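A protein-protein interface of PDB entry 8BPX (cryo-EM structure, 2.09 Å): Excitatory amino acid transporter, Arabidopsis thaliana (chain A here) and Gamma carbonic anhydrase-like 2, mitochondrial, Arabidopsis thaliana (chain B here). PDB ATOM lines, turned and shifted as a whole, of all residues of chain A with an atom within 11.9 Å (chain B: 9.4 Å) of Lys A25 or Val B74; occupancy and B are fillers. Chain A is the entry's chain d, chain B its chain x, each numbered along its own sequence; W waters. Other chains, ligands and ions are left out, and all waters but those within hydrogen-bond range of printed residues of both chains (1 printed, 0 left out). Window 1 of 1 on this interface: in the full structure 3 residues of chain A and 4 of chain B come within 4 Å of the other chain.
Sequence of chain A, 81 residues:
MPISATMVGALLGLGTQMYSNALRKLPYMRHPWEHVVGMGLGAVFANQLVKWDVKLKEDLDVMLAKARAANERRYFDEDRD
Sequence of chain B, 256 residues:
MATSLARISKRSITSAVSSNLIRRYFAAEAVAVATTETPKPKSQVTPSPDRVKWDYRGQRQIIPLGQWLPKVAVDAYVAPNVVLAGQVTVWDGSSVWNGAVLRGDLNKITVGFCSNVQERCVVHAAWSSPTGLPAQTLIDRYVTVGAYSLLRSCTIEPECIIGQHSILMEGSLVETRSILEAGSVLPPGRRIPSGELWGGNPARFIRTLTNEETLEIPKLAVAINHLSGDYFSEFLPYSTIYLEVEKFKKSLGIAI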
ATOM      1  N   THR A  16     -16.011  10.369 -24.470  1.00  0.00           N
ATOM      2  CA  THR A  16     -15.758  11.365 -25.524  1.00  0.00           C
ATOM      3  C   THR A  16     -16.326  12.722 -25.095  1.00  0.00           C
ATOM      4  O   THR A  16     -15.583  13.643 -25.138  1.00  0.00           O
ATOM      5  CB  THR A  16     -16.182  10.867 -26.916  1.00  0.00           C
ATOM      6  OG1 THR A  16     -15.448   9.703 -27.294  1.00  0.00           O
ATOM      7  CG2 THR A  16     -16.001  11.924 -27.984  1.00  0.00           C
ATOM      8  N   GLN A  17     -17.568  12.760 -24.638  1.00  0.00           N
ATOM      9  CA  GLN A  17     -18.227  13.988 -24.157  1.00  0.00           C
ATOM     10  C   GLN A  17     -17.423  14.618 -23.006  1.00  0.00           C
ATOM     11  O   GLN A  17     -17.058  15.759 -23.118  1.00  0.00           O
ATOM     12  CB  GLN A  17     -19.712  13.746 -23.779  1.00  0.00           C
ATOM     13  CG  GLN A  17     -20.444  14.952 -23.216  1.00  0.00           C
ATOM     14  CD  GLN A  17     -20.446  16.218 -24.048  1.00  0.00           C
ATOM     15  OE1 GLN A  17     -20.229  16.208 -25.256  1.00  0.00           O
ATOM     16  NE2 GLN A  17     -20.713  17.330 -23.382  1.00  0.00           N
ATOM     17  N   MET A  18     -17.069  13.829 -22.021  1.00  0.00           N
ATOM     18  CA  MET A  18     -16.273  14.300 -20.854  1.00  0.00           C
ATOM     19  C   MET A  18     -14.902  14.848 -21.276  1.00  0.00           C
ATOM     20  O   MET A  18     -14.581  15.897 -20.836  1.00  0.00           O
ATOM     21  CB  MET A  18     -16.109  13.148 -19.857  1.00  0.00           C
ATOM     22  CG  MET A  18     -17.449  12.671 -19.311  1.00  0.00           C
ATOM     23  SD  MET A  18     -17.358  11.340 -18.094  1.00  0.00           S
ATOM     24  CE  MET A  18     -17.124  12.306 -16.607  1.00  0.00           C
ATOM     25  N   TYR A  19     -14.167  14.112 -22.097  1.00  0.00           N
ATOM     26  CA  TYR A  19     -12.874  14.512 -22.656  1.00  0.00           C
ATOM     27  C   TYR A  19     -13.063  15.845 -23.419  1.00  0.00           C
ATOM     28  O   TYR A  19     -12.291  16.736 -23.226  1.00  0.00           O
ATOM     29  CB  TYR A  19     -12.324  13.364 -23.523  1.00  0.00           C
ATOM     30  CG  TYR A  19     -10.886  13.363 -23.917  1.00  0.00           C
ATOM     31  CD1 TYR A  19     -10.018  14.385 -23.580  1.00  0.00           C
ATOM     32  CD2 TYR A  19     -10.393  12.272 -24.606  1.00  0.00           C
ATOM     33  CE1 TYR A  19      -8.688  14.327 -23.949  1.00  0.00           C
ATOM     34  CE2 TYR A  19      -9.071  12.199 -24.975  1.00  0.00           C
ATOM     35  CZ  TYR A  19      -8.225  13.245 -24.672  1.00  0.00           C
ATOM     36  OH  TYR A  19      -6.924  13.134 -25.036  1.00  0.00           O
ATOM     37  N   SER A  20     -14.070  15.909 -24.269  1.00  0.00           N
ATOM     38  CA  SER A  20     -14.400  17.182 -24.989  1.00  0.00           C
ATOM     39  C   SER A  20     -14.632  18.355 -23.991  1.00  0.00           C
ATOM     40  O   SER A  20     -13.986  19.360 -24.158  1.00  0.00           O
ATOM     41  CB  SER A  20     -15.536  17.039 -25.928  1.00  0.00           C
ATOM     42  OG  SER A  20     -15.989  18.269 -26.419  1.00  0.00           O
ATOM     43  N   ASN A  21     -15.456  18.169 -22.977  1.00  0.00           N
ATOM     44  CA  ASN A  21     -15.684  19.185 -21.903  1.00  0.00           C
ATOM     45  C   ASN A  21     -14.367  19.581 -21.230  1.00  0.00           C
ATOM     46  O   ASN A  21     -14.116  20.774 -21.107  1.00  0.00           O
ATOM     47  CB  ASN A  21     -16.738  18.706 -20.884  1.00  0.00           C
ATOM     48  CG  ASN A  21     -18.177  18.968 -21.290  1.00  0.00           C
ATOM     49  OD1 ASN A  21     -18.442  19.702 -22.229  1.00  0.00           O
ATOM     50  ND2 ASN A  21     -19.119  18.358 -20.597  1.00  0.00           N
ATOM     51  N   ALA A  22     -13.579  18.605 -20.853  1.00  0.00           N
ATOM     52  CA  ALA A  22     -12.300  18.846 -20.178  1.00  0.00           C
ATOM     53  C   ALA A  22     -11.348  19.657 -21.073  1.00  0.00           C
ATOM     54  O   ALA A  22     -10.768  20.561 -20.561  1.00  0.00           O
ATOM     55  CB  ALA A  22     -11.694  17.568 -19.754  1.00  0.00           C
ATOM     56  N   LEU A  23     -11.247  19.265 -22.324  1.00  0.00           N
ATOM     57  CA  LEU A  23     -10.399  20.007 -23.275  1.00  0.00           C
ATOM     58  C   LEU A  23     -10.797  21.465 -23.350  1.00  0.00           C
ATOM     59  O   LEU A  23      -9.943  22.242 -23.538  1.00  0.00           O
ATOM     60  CB  LEU A  23     -10.368  19.379 -24.666  1.00  0.00           C
ATOM     61  CG  LEU A  23      -9.528  18.111 -24.780  1.00  0.00           C
ATOM     62  CD1 LEU A  23      -9.925  17.302 -26.001  1.00  0.00           C
ATOM     63  CD2 LEU A  23      -8.036  18.427 -24.782  1.00  0.00           C
ATOM     64  N   ARG A  24     -12.077  21.745 -23.213  1.00  0.00           N
ATOM     65  CA  ARG A  24     -12.571  23.113 -23.241  1.00  0.00           C
ATOM     66  C   ARG A  24     -12.566  23.764 -21.863  1.00  0.00           C
ATOM     67  O   ARG A  24     -13.136  24.849 -21.702  1.00  0.00           O
ATOM     68  CB  ARG A  24     -13.977  23.143 -23.842  1.00  0.00           C
ATOM     69  CG  ARG A  24     -14.029  22.555 -25.241  1.00  0.00           C
ATOM     70  CD  ARG A  24     -15.439  22.212 -25.662  1.00  0.00           C
ATOM     71  NE  ARG A  24     -16.296  23.387 -25.692  1.00  0.00           N
ATOM     72  CZ  ARG A  24     -17.606  23.361 -25.497  1.00  0.00           C
ATOM     73  NH1 ARG A  24     -18.246  22.229 -25.258  1.00  0.00           N
ATOM     74  NH2 ARG A  24     -18.290  24.500 -25.543  1.00  0.00           N
ATOM     75  N   LYS A  25     -11.942  23.123 -20.873  1.00  0.00           N
ATOM     76  CA  LYS A  25     -11.842  23.639 -19.507  1.00  0.00           C
ATOM     77  C   LYS A  25     -13.214  23.856 -18.872  1.00  0.00           C
ATOM     78  O   LYS A  25     -13.392  24.749 -18.045  1.00  0.00           O
ATOM     79  CB  LYS A  25     -11.016  24.930 -19.456  1.00  0.00           C
ATOM     80  CG  LYS A  25      -9.762  24.896 -20.317  1.00  0.00           C
ATOM     81  CD  LYS A  25      -8.635  25.692 -19.691  1.00  0.00           C
ATOM     82  CE  LYS A  25      -8.076  24.995 -18.467  1.00  0.00           C
ATOM     83  NZ  LYS A  25      -7.332  25.940 -17.595  1.00  0.00           N
ATOM     84  N   LEU A  26     -14.179  23.040 -19.251  1.00  0.00           N
ATOM     85  CA  LEU A  26     -15.518  23.040 -18.696  1.00  0.00           C
ATOM     86  C   LEU A  26     -15.683  21.903 -17.699  1.00  0.00           C
ATOM     87  O   LEU A  26     -14.915  20.938 -17.709  1.00  0.00           O
ATOM     88  CB  LEU A  26     -16.559  22.902 -19.812  1.00  0.00           C
ATOM     89  CG  LEU A  26     -16.629  24.044 -20.826  1.00  0.00           C
ATOM     90  CD1 LEU A  26     -17.577  23.684 -21.965  1.00  0.00           C
ATOM     91  CD2 LEU A  26     -17.046  25.342 -20.156  1.00  0.00           C
ATOM     92  N   PRO A  27     -16.666  21.996 -16.805  1.00  0.00           N
ATOM     93  CA  PRO A  27     -16.951  20.867 -15.909  1.00  0.00           C
ATOM     94  C   PRO A  27     -17.305  19.619 -16.703  1.00  0.00           C
ATOM     95  O   PRO A  27     -17.879  19.692 -17.791  1.00  0.00           O
ATOM     96  CB  PRO A  27     -18.144  21.355 -15.079  1.00  0.00           C
ATOM     97  CG  PRO A  27     -18.123  22.834 -15.177  1.00  0.00           C
ATOM     98  CD  PRO A  27     -17.382  23.224 -16.417  1.00  0.00           C
ATOM     99  N   TYR A  28     -16.940  18.462 -16.142  1.00  0.00           N
ATOM    100  CA  TYR A  28     -17.139  17.187 -16.828  1.00  0.00           C
ATOM    101  C   TYR A  28     -18.572  17.014 -17.312  1.00  0.00           C
ATOM    102  O   TYR A  28     -18.804  16.532 -18.423  1.00  0.00           O
ATOM    103  CB  TYR A  28     -16.761  16.028 -15.904  1.00  0.00           C
ATOM    104  CG  TYR A  28     -15.283  15.731 -15.837  1.00  0.00           C
ATOM    105  CD1 TYR A  28     -14.537  15.543 -16.992  1.00  0.00           C
ATOM    106  CD2 TYR A  28     -14.635  15.625 -14.615  1.00  0.00           C
ATOM    107  CE1 TYR A  28     -13.187  15.259 -16.931  1.00  0.00           C
ATOM    108  CE2 TYR A  28     -13.286  15.342 -14.544  1.00  0.00           C
ATOM    109  CZ  TYR A  28     -12.567  15.162 -15.702  1.00  0.00           C
ATOM    110  OH  TYR A  28     -11.224  14.883 -15.636  1.00  0.00           O
ATOM    111  N   MET A  29     -19.545  17.406 -16.496  1.00  0.00           N
ATOM    112  CA  MET A  29     -20.954  17.156 -16.774  1.00  0.00           C
ATOM    113  C   MET A  29     -21.700  18.431 -17.156  1.00  0.00           C
ATOM    114  O   MET A  29     -22.855  18.623 -16.777  1.00  0.00           O
ATOM    115  CB  MET A  29     -21.615  16.481 -15.578  1.00  0.00           C
ATOM    116  CG  MET A  29     -20.832  15.300 -15.052  1.00  0.00           C
ATOM    117  SD  MET A  29     -21.116  13.818 -16.036  1.00  0.00           S
ATOM    118  CE  MET A  29     -22.848  13.994 -16.457  1.00  0.00           C
ATOM    119  N   ARG A  30     -21.048  19.303 -17.928  1.00  0.00           N
ATOM    120  CA  ARG A  30     -21.608  20.621 -18.213  1.00  0.00           C
ATOM    121  C   ARG A  30     -22.980  20.520 -18.879  1.00  0.00           C
ATOM    122  O   ARG A  30     -23.934  21.155 -18.433  1.00  0.00           O
ATOM    123  CB  ARG A  30     -20.631  21.432 -19.067  1.00  0.00           C
ATOM    124  CG  ARG A  30     -21.214  22.637 -19.818  1.00  0.00           C
ATOM    125  CD  ARG A  30     -22.058  23.605 -18.974  1.00  0.00           C
ATOM    126  NE  ARG A  30     -21.461  23.963 -17.695  1.00  0.00           N
ATOM    127  CZ  ARG A  30     -20.810  25.096 -17.471  1.00  0.00           C
ATOM    128  NH1 ARG A  30     -20.560  25.954 -18.446  1.00  0.00           N
ATOM    129  NH2 ARG A  30     -20.391  25.372 -16.239  1.00  0.00           N
ATOM    130  N   HIS A  31     -23.110  19.731 -19.942  1.00  0.00           N
ATOM    131  CA  HIS A  31     -24.403  19.563 -20.615  1.00  0.00           C
ATOM    132  C   HIS A  31     -24.765  18.082 -20.618  1.00  0.00           C
ATOM    133  O   HIS A  31     -24.455  17.362 -21.577  1.00  0.00           O
ATOM    134  CB  HIS A  31     -24.366  20.127 -22.036  1.00  0.00           C
ATOM    135  CG  HIS A  31     -24.451  21.620 -22.103  1.00  0.00           C
ATOM    136  ND1 HIS A  31     -24.288  22.320 -23.280  1.00  0.00           N
ATOM    137  CD2 HIS A  31     -24.696  22.547 -21.147  1.00  0.00           C
ATOM    138  CE1 HIS A  31     -24.422  23.613 -23.043  1.00  0.00           C
ATOM    139  NE2 HIS A  31     -24.668  23.777 -21.757  1.00  0.00           N
ATOM    140  N   HIS A  35     -24.102  14.076 -22.819  1.00  0.00           N
ATOM    141  CA  HIS A  35     -23.524  12.804 -22.399  1.00  0.00           C
ATOM    142  C   HIS A  35     -24.426  11.641 -22.789  1.00  0.00           C
ATOM    143  O   HIS A  35     -23.946  10.589 -23.232  1.00  0.00           O
ATOM    144  CB  HIS A  35     -23.274  12.811 -20.891  1.00  0.00           C
ATOM    145  CG  HIS A  35     -22.292  13.848 -20.446  1.00  0.00           C
ATOM    146  ND1 HIS A  35     -22.542  15.199 -20.537  1.00  0.00           N
ATOM    147  CD2 HIS A  35     -21.060  13.730 -19.895  1.00  0.00           C
ATOM    148  CE1 HIS A  35     -21.506  15.869 -20.068  1.00  0.00           C
ATOM    149  NE2 HIS A  35     -20.594  15.002 -19.671  1.00  0.00           N
ATOM    150  N   LYS B  71     -12.936  40.494 -19.395  1.00  0.00           N
ATOM    151  CA  LYS B  71     -12.734  39.145 -19.908  1.00  0.00           C
ATOM    152  C   LYS B  71     -12.481  38.201 -18.740  1.00  0.00           C
ATOM    153  O   LYS B  71     -11.502  38.368 -18.005  1.00  0.00           O
ATOM    154  CB  LYS B  71     -11.562  39.109 -20.890  1.00  0.00           C
ATOM    155  CG  LYS B  71     -11.223  37.721 -21.420  1.00  0.00           C
ATOM    156  CD  LYS B  71     -10.088  37.788 -22.426  1.00  0.00           C
ATOM    157  CE  LYS B  71      -9.480  36.415 -22.673  1.00  0.00           C
ATOM    158  NZ  LYS B  71      -8.270  36.169 -21.842  1.00  0.00           N
ATOM    159  N   VAL B  72     -13.352  37.210 -18.580  1.00  0.00           N
ATOM    160  CA  VAL B  72     -13.284  36.250 -17.484  1.00  0.00           C
ATOM    161  C   VAL B  72     -13.108  34.855 -18.067  1.00  0.00           C
ATOM    162  O   VAL B  72     -13.908  34.422 -18.901  1.00  0.00           O
ATOM    163  CB  VAL B  72     -14.542  36.318 -16.596  1.00  0.00           C
ATOM    164  CG1 VAL B  72     -14.421  35.364 -15.418  1.00  0.00           C
ATOM    165  CG2 VAL B  72     -14.783  37.744 -16.119  1.00  0.00           C
ATOM    166  N   ALA B  73     -12.067  34.156 -17.625  1.00  0.00           N
ATOM    167  CA  ALA B  73     -11.836  32.789 -18.070  1.00  0.00           C
ATOM    168  C   ALA B  73     -12.958  31.869 -17.595  1.00  0.00           C
ATOM    169  O   ALA B  73     -13.541  32.064 -16.526  1.00  0.00           O
ATOM    170  CB  ALA B  73     -10.485  32.280 -17.563  1.00  0.00           C
ATOM    171  N   VAL B  74     -13.258  30.853 -18.410  1.00  0.00           N
ATOM    172  CA  VAL B  74     -14.373  29.960 -18.110  1.00  0.00           C
ATOM    173  C   VAL B  74     -14.136  29.154 -16.838  1.00  0.00           C
ATOM    174  O   VAL B  74     -15.102  28.706 -16.211  1.00  0.00           O
ATOM    175  CB  VAL B  74     -14.656  29.026 -19.303  1.00  0.00           C
ATOM    176  CG1 VAL B  74     -14.974  29.844 -20.543  1.00  0.00           C
ATOM    177  CG2 VAL B  74     -13.478  28.085 -19.556  1.00  0.00           C
ATOM    178  N   ASP B  75     -12.880  28.959 -16.435  1.00  0.00           N
ATOM    179  CA  ASP B  75     -12.545  28.237 -15.215  1.00  0.00           C
ATOM    180  C   ASP B  75     -12.042  29.169 -14.115  1.00  0.00           C
ATOM    181  O   ASP B  75     -11.185  28.789 -13.315  1.00  0.00           O
ATOM    182  CB  ASP B  75     -11.510  27.154 -15.505  1.00  0.00           C
ATOM    183  CG  ASP B  75     -10.187  27.725 -15.976  1.00  0.00           C
ATOM    184  OD1 ASP B  75      -9.133  27.153 -15.634  1.00  0.00           O
ATOM    185  OD2 ASP B  75     -10.203  28.756 -16.678  1.00  0.00           O
ATOM    186  N   ALA B  76     -12.549  30.396 -14.075  1.00  0.00           N
ATOM    187  CA  ALA B  76     -12.257  31.339 -13.008  1.00  0.00           C
ATOM    188  C   ALA B  76     -13.526  31.607 -12.210  1.00  0.00           C
ATOM    189  O   ALA B  76     -14.617  31.696 -12.782  1.00  0.00           O
ATOM    190  CB  ALA B  76     -11.697  32.651 -13.563  1.00  0.00           C
ATOM    191  N   TYR B  77     -13.387  31.724 -10.895  1.00  0.00           N
ATOM    192  CA  TYR B  77     -14.511  32.032 -10.021  1.00  0.00           C
ATOM    193  C   TYR B  77     -14.559  33.531  -9.761  1.00  0.00           C
ATOM    194  O   TYR B  77     -13.588  34.111  -9.269  1.00  0.00           O
ATOM    195  CB  TYR B  77     -14.421  31.283  -8.693  1.00  0.00           C
ATOM    196  CG  TYR B  77     -15.511  31.699  -7.732  1.00  0.00           C
ATOM    197  CD1 TYR B  77     -16.841  31.431  -8.013  1.00  0.00           C
ATOM    198  CD2 TYR B  77     -15.215  32.390  -6.562  1.00  0.00           C
ATOM    199  CE1 TYR B  77     -17.847  31.816  -7.153  1.00  0.00           C
ATOM    200  CE2 TYR B  77     -16.221  32.782  -5.690  1.00  0.00           C
ATOM    201  CZ  TYR B  77     -17.534  32.492  -5.997  1.00  0.00           C
ATOM    202  OH  TYR B  77     -18.546  32.872  -5.150  1.00  0.00           O
ATOM    203  N   VAL B  78     -15.688  34.153 -10.079  1.00  0.00           N
ATOM    204  CA  VAL B  78     -15.944  35.546  -9.737  1.00  0.00           C
ATOM    205  C   VAL B  78     -17.223  35.586  -8.913  1.00  0.00           C
ATOM    206  O   VAL B  78     -18.285  35.168  -9.389  1.00  0.00           O
ATOM    207  CB  VAL B  78     -16.054  36.437 -10.985  1.00  0.00           C
ATOM    208  CG1 VAL B  78     -16.353  37.870 -10.583  1.00  0.00           C
ATOM    209  CG2 VAL B  78     -14.770  36.363 -11.801  1.00  0.00           C
ATOM    210  N   VAL B  90      -9.389  38.436 -16.236  1.00  0.00           N
ATOM    211  CA  VAL B  90      -9.309  37.470 -15.148  1.00  0.00           C
ATOM    212  C   VAL B  90      -9.002  36.112 -15.772  1.00  0.00           C
ATOM    213  O   VAL B  90      -9.826  35.569 -16.518  1.00  0.00           O
ATOM    214  CB  VAL B  90     -10.615  37.448 -14.332  1.00  0.00           C
ATOM    215  CG1 VAL B  90     -10.649  36.294 -13.368  1.00  0.00           C
ATOM    216  CG2 VAL B  90     -10.800  38.775 -13.597  1.00  0.00           C
ATOM    217  N   TRP B  91      -7.826  35.566 -15.466  1.00  0.00           N
ATOM    218  CA  TRP B  91      -7.277  34.437 -16.203  1.00  0.00           C
ATOM    219  C   TRP B  91      -7.656  33.103 -15.553  1.00  0.00           C
ATOM    220  O   TRP B  91      -8.311  33.051 -14.513  1.00  0.00           O
ATOM    221  CB  TRP B  91      -5.762  34.580 -16.326  1.00  0.00           C
ATOM    222  CG  TRP B  91      -5.344  35.539 -17.394  1.00  0.00           C
ATOM    223  CD1 TRP B  91      -4.886  36.811 -17.219  1.00  0.00           C
ATOM    224  CD2 TRP B  91      -5.354  35.310 -18.809  1.00  0.00           C
ATOM    225  NE1 TRP B  91      -4.607  37.387 -18.433  1.00  0.00           N
ATOM    226  CE2 TRP B  91      -4.888  36.485 -19.425  1.00  0.00           C
ATOM    227  CE3 TRP B  91      -5.715  34.223 -19.614  1.00  0.00           C
ATOM    228  CZ2 TRP B  91      -4.767  36.606 -20.808  1.00  0.00           C
ATOM    229  CZ3 TRP B  91      -5.594  34.344 -20.985  1.00  0.00           C
ATOM    230  CH2 TRP B  91      -5.124  35.528 -21.568  1.00  0.00           C
ATOM    231  N   ASP B  92      -7.224  32.011 -16.184  1.00  0.00           N
ATOM    232  CA  ASP B  92      -7.608  30.672 -15.754  1.00  0.00           C
ATOM    233  C   ASP B  92      -7.151  30.385 -14.328  1.00  0.00           C
ATOM    234  O   ASP B  92      -6.018  30.690 -13.945  1.00  0.00           O
ATOM    235  CB  ASP B  92      -7.023  29.621 -16.700  1.00  0.00           C
ATOM    236  CG  ASP B  92      -7.692  29.620 -18.059  1.00  0.00           C
ATOM    237  OD1 ASP B  92      -8.781  30.216 -18.196  1.00  0.00           O
ATOM    238  OD2 ASP B  92      -7.128  29.012 -18.990  1.00  0.00           O
ATOM    239  N   GLY B  93      -8.052  29.796 -13.543  1.00  0.00           N
ATOM    240  CA  GLY B  93      -7.749  29.369 -12.196  1.00  0.00           C
ATOM    241  C   GLY B  93      -7.774  30.461 -11.152  1.00  0.00           C
ATOM    242  O   GLY B  93      -7.608  30.162  -9.965  1.00  0.00           O
ATOM    243  N   SER B  94      -7.988  31.709 -11.548  1.00  0.00           N
ATOM    244  CA  SER B  94      -8.012  32.807 -10.602  1.00  0.00           C
ATOM    245  C   SER B  94      -9.399  32.948  -9.970  1.00  0.00           C
ATOM    246  O   SER B  94     -10.382  32.358 -10.423  1.00  0.00           O
ATOM    247  CB  SER B  94      -7.580  34.104 -11.283  1.00  0.00           C
ATOM    248  OG  SER B  94      -8.523  34.510 -12.245  1.00  0.00           O
ATOM    249  N   PHE B 113      -2.677  33.773 -13.708  1.00  0.00           N
ATOM    250  CA  PHE B 113      -3.006  32.362 -13.554  1.00  0.00           C
ATOM    251  C   PHE B 113      -2.965  31.949 -12.088  1.00  0.00           C
ATOM    252  O   PHE B 113      -1.957  32.153 -11.406  1.00  0.00           O
ATOM    253  CB  PHE B 113      -2.030  31.514 -14.369  1.00  0.00           C
ATOM    254  CG  PHE B 113      -2.211  30.034 -14.188  1.00  0.00           C
ATOM    255  CD1 PHE B 113      -3.239  29.363 -14.825  1.00  0.00           C
ATOM    256  CD2 PHE B 113      -1.355  29.316 -13.368  1.00  0.00           C
ATOM    257  CE1 PHE B 113      -3.405  27.999 -14.657  1.00  0.00           C
ATOM    258  CE2 PHE B 113      -1.518  27.956 -13.196  1.00  0.00           C
ATOM    259  CZ  PHE B 113      -2.544  27.298 -13.840  1.00  0.00           C
ATOM    260  N   CYS B 114      -4.067  31.369 -11.613  1.00  0.00           N
ATOM    261  CA  CYS B 114      -4.159  30.806 -10.265  1.00  0.00           C
ATOM    262  C   CYS B 114      -3.891  31.848  -9.180  1.00  0.00           C
ATOM    263  O   CYS B 114      -3.356  31.526  -8.119  1.00  0.00           O
ATOM    264  CB  CYS B 114      -3.212  29.612 -10.103  1.00  0.00           C
ATOM    265  SG  CYS B 114      -3.818  28.327  -8.994  1.00  0.00           S
ATOM    266  N   ASN B 225      -7.354  28.341  -4.838  1.00  0.00           N
ATOM    267  CA  ASN B 225      -8.069  27.934  -6.048  1.00  0.00           C
ATOM    268  C   ASN B 225      -8.938  26.702  -5.789  1.00  0.00           C
ATOM    269  O   ASN B 225     -10.083  26.617  -6.263  1.00  0.00           O
ATOM    270  CB  ASN B 225      -7.074  27.675  -7.182  1.00  0.00           C
ATOM    271  CG  ASN B 225      -7.671  26.857  -8.313  1.00  0.00           C
ATOM    272  OD1 ASN B 225      -7.665  25.628  -8.276  1.00  0.00           O
ATOM    273  ND2 ASN B 225      -8.195  27.537  -9.325  1.00  0.00           N
ATOM    274  N   PHE B 232     -17.533  27.730  -7.143  1.00  0.00           N
ATOM    275  CA  PHE B 232     -17.846  27.678  -8.567  1.00  0.00           C
ATOM    276  C   PHE B 232     -18.889  26.608  -8.859  1.00  0.00           C
ATOM    277  O   PHE B 232     -19.788  26.814  -9.681  1.00  0.00           O
ATOM    278  CB  PHE B 232     -16.571  27.421  -9.371  1.00  0.00           C
ATOM    279  CG  PHE B 232     -16.761  27.486 -10.859  1.00  0.00           C
ATOM    280  CD1 PHE B 232     -17.175  26.370 -11.572  1.00  0.00           C
ATOM    281  CD2 PHE B 232     -16.516  28.662 -11.549  1.00  0.00           C
ATOM    282  CE1 PHE B 232     -17.348  26.429 -12.943  1.00  0.00           C
ATOM    283  CE2 PHE B 232     -16.684  28.727 -12.918  1.00  0.00           C
ATOM    284  CZ  PHE B 232     -17.103  27.609 -13.615  1.00  0.00           C
ATOM    285  N   SER B 233     -18.806  25.462  -8.230  1.00  0.00           N
ATOM    286  CA  SER B 233     -19.773  24.341  -8.403  1.00  0.00           C
ATOM    287  C   SER B 233     -21.194  24.643  -7.881  1.00  0.00           C
ATOM    288  O   SER B 233     -22.094  23.922  -8.274  1.00  0.00           O
ATOM    289  CB  SER B 233     -19.165  23.065  -7.848  1.00  0.00           C
ATOM    290  OG  SER B 233     -17.961  22.747  -8.510  1.00  0.00           O
ATOM    291  N   PHE B 235     -23.000  27.265  -8.777  1.00  0.00           N
ATOM    292  CA  PHE B 235     -23.725  28.114  -9.715  1.00  0.00           C
ATOM    293  C   PHE B 235     -23.872  27.403 -11.052  1.00  0.00           C
ATOM    294  O   PHE B 235     -22.874  27.037 -11.678  1.00  0.00           O
ATOM    295  CB  PHE B 235     -23.008  29.455  -9.902  1.00  0.00           C
ATOM    296  CG  PHE B 235     -22.974  30.297  -8.663  1.00  0.00           C
ATOM    297  CD1 PHE B 235     -24.030  31.136  -8.349  1.00  0.00           C
ATOM    298  CD2 PHE B 235     -21.887  30.244  -7.803  1.00  0.00           C
ATOM    299  CE1 PHE B 235     -24.001  31.909  -7.208  1.00  0.00           C
ATOM    300  CE2 PHE B 235     -21.854  31.013  -6.659  1.00  0.00           C
ATOM    301  CZ  PHE B 235     -22.912  31.849  -6.362  1.00  0.00           C
HETATM  302  O   HOH W   1     -15.112  25.783 -16.180  1.00  0.00           O
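Among the printed residues, merely in contact across the chains: Arg A24 with Val B74 (3.9 Å) and Lys A25 with Val B74 (3.7 Å).
The side-chain carboxylate (OD2) of Asp B92 lies within salt-bridge range of the side-chain amino group (NZ) of Lys A25, at 3.4 Å.
OD1 of Asp B75 lies within salt-bridge range of NZ of Lys A25 (2.9 Å).
The backbone carbonyl oxygen (O) of Asp B92 lies within hydrogen-bond range of the backbone NH (N) of Cys B114.
The backbone carbonyl oxygen of Asp B75 lies within hydrogen-bond range of the backbone NH of Gly B93, at 3.3 Å.
The side-chain carboxylate of Asp B75 sits close to the side-chain carboxylate of Asp B92, at 2.5 Å.
Of the 17 printed residues of chain A, 2 touch a printed residue of chain B.
Printed residues of chain B that touch a printed residue of chain A: Val B74, Asp B75 and Asp B92.
Hydrophobic or aromatic side chains of chain B that line the printed part of chain A: Val B74.
Among the printed residues, 4 pairs touch across the chains.
Of chain B, only Val B74 (3.7 Å), Asp B75 (2.9 Å) and Asp B92 (3.4 Å) come within 4 Å of Lys A25.
Val B74 touches two residues of chain A.
No residue of chain A comes within 4 Å of Val B72.
Of chain A, only Lys A25 (2.9 Å) comes within 4 Å of Asp B75.
Printed residues of chain B within 4 Å of Arg A24: Val B74 (3.9 Å).
Water W1 lies within hydrogen-bond range of O of Lys A25 (2.7 Å) and O of Val B74 (2.9 Å).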
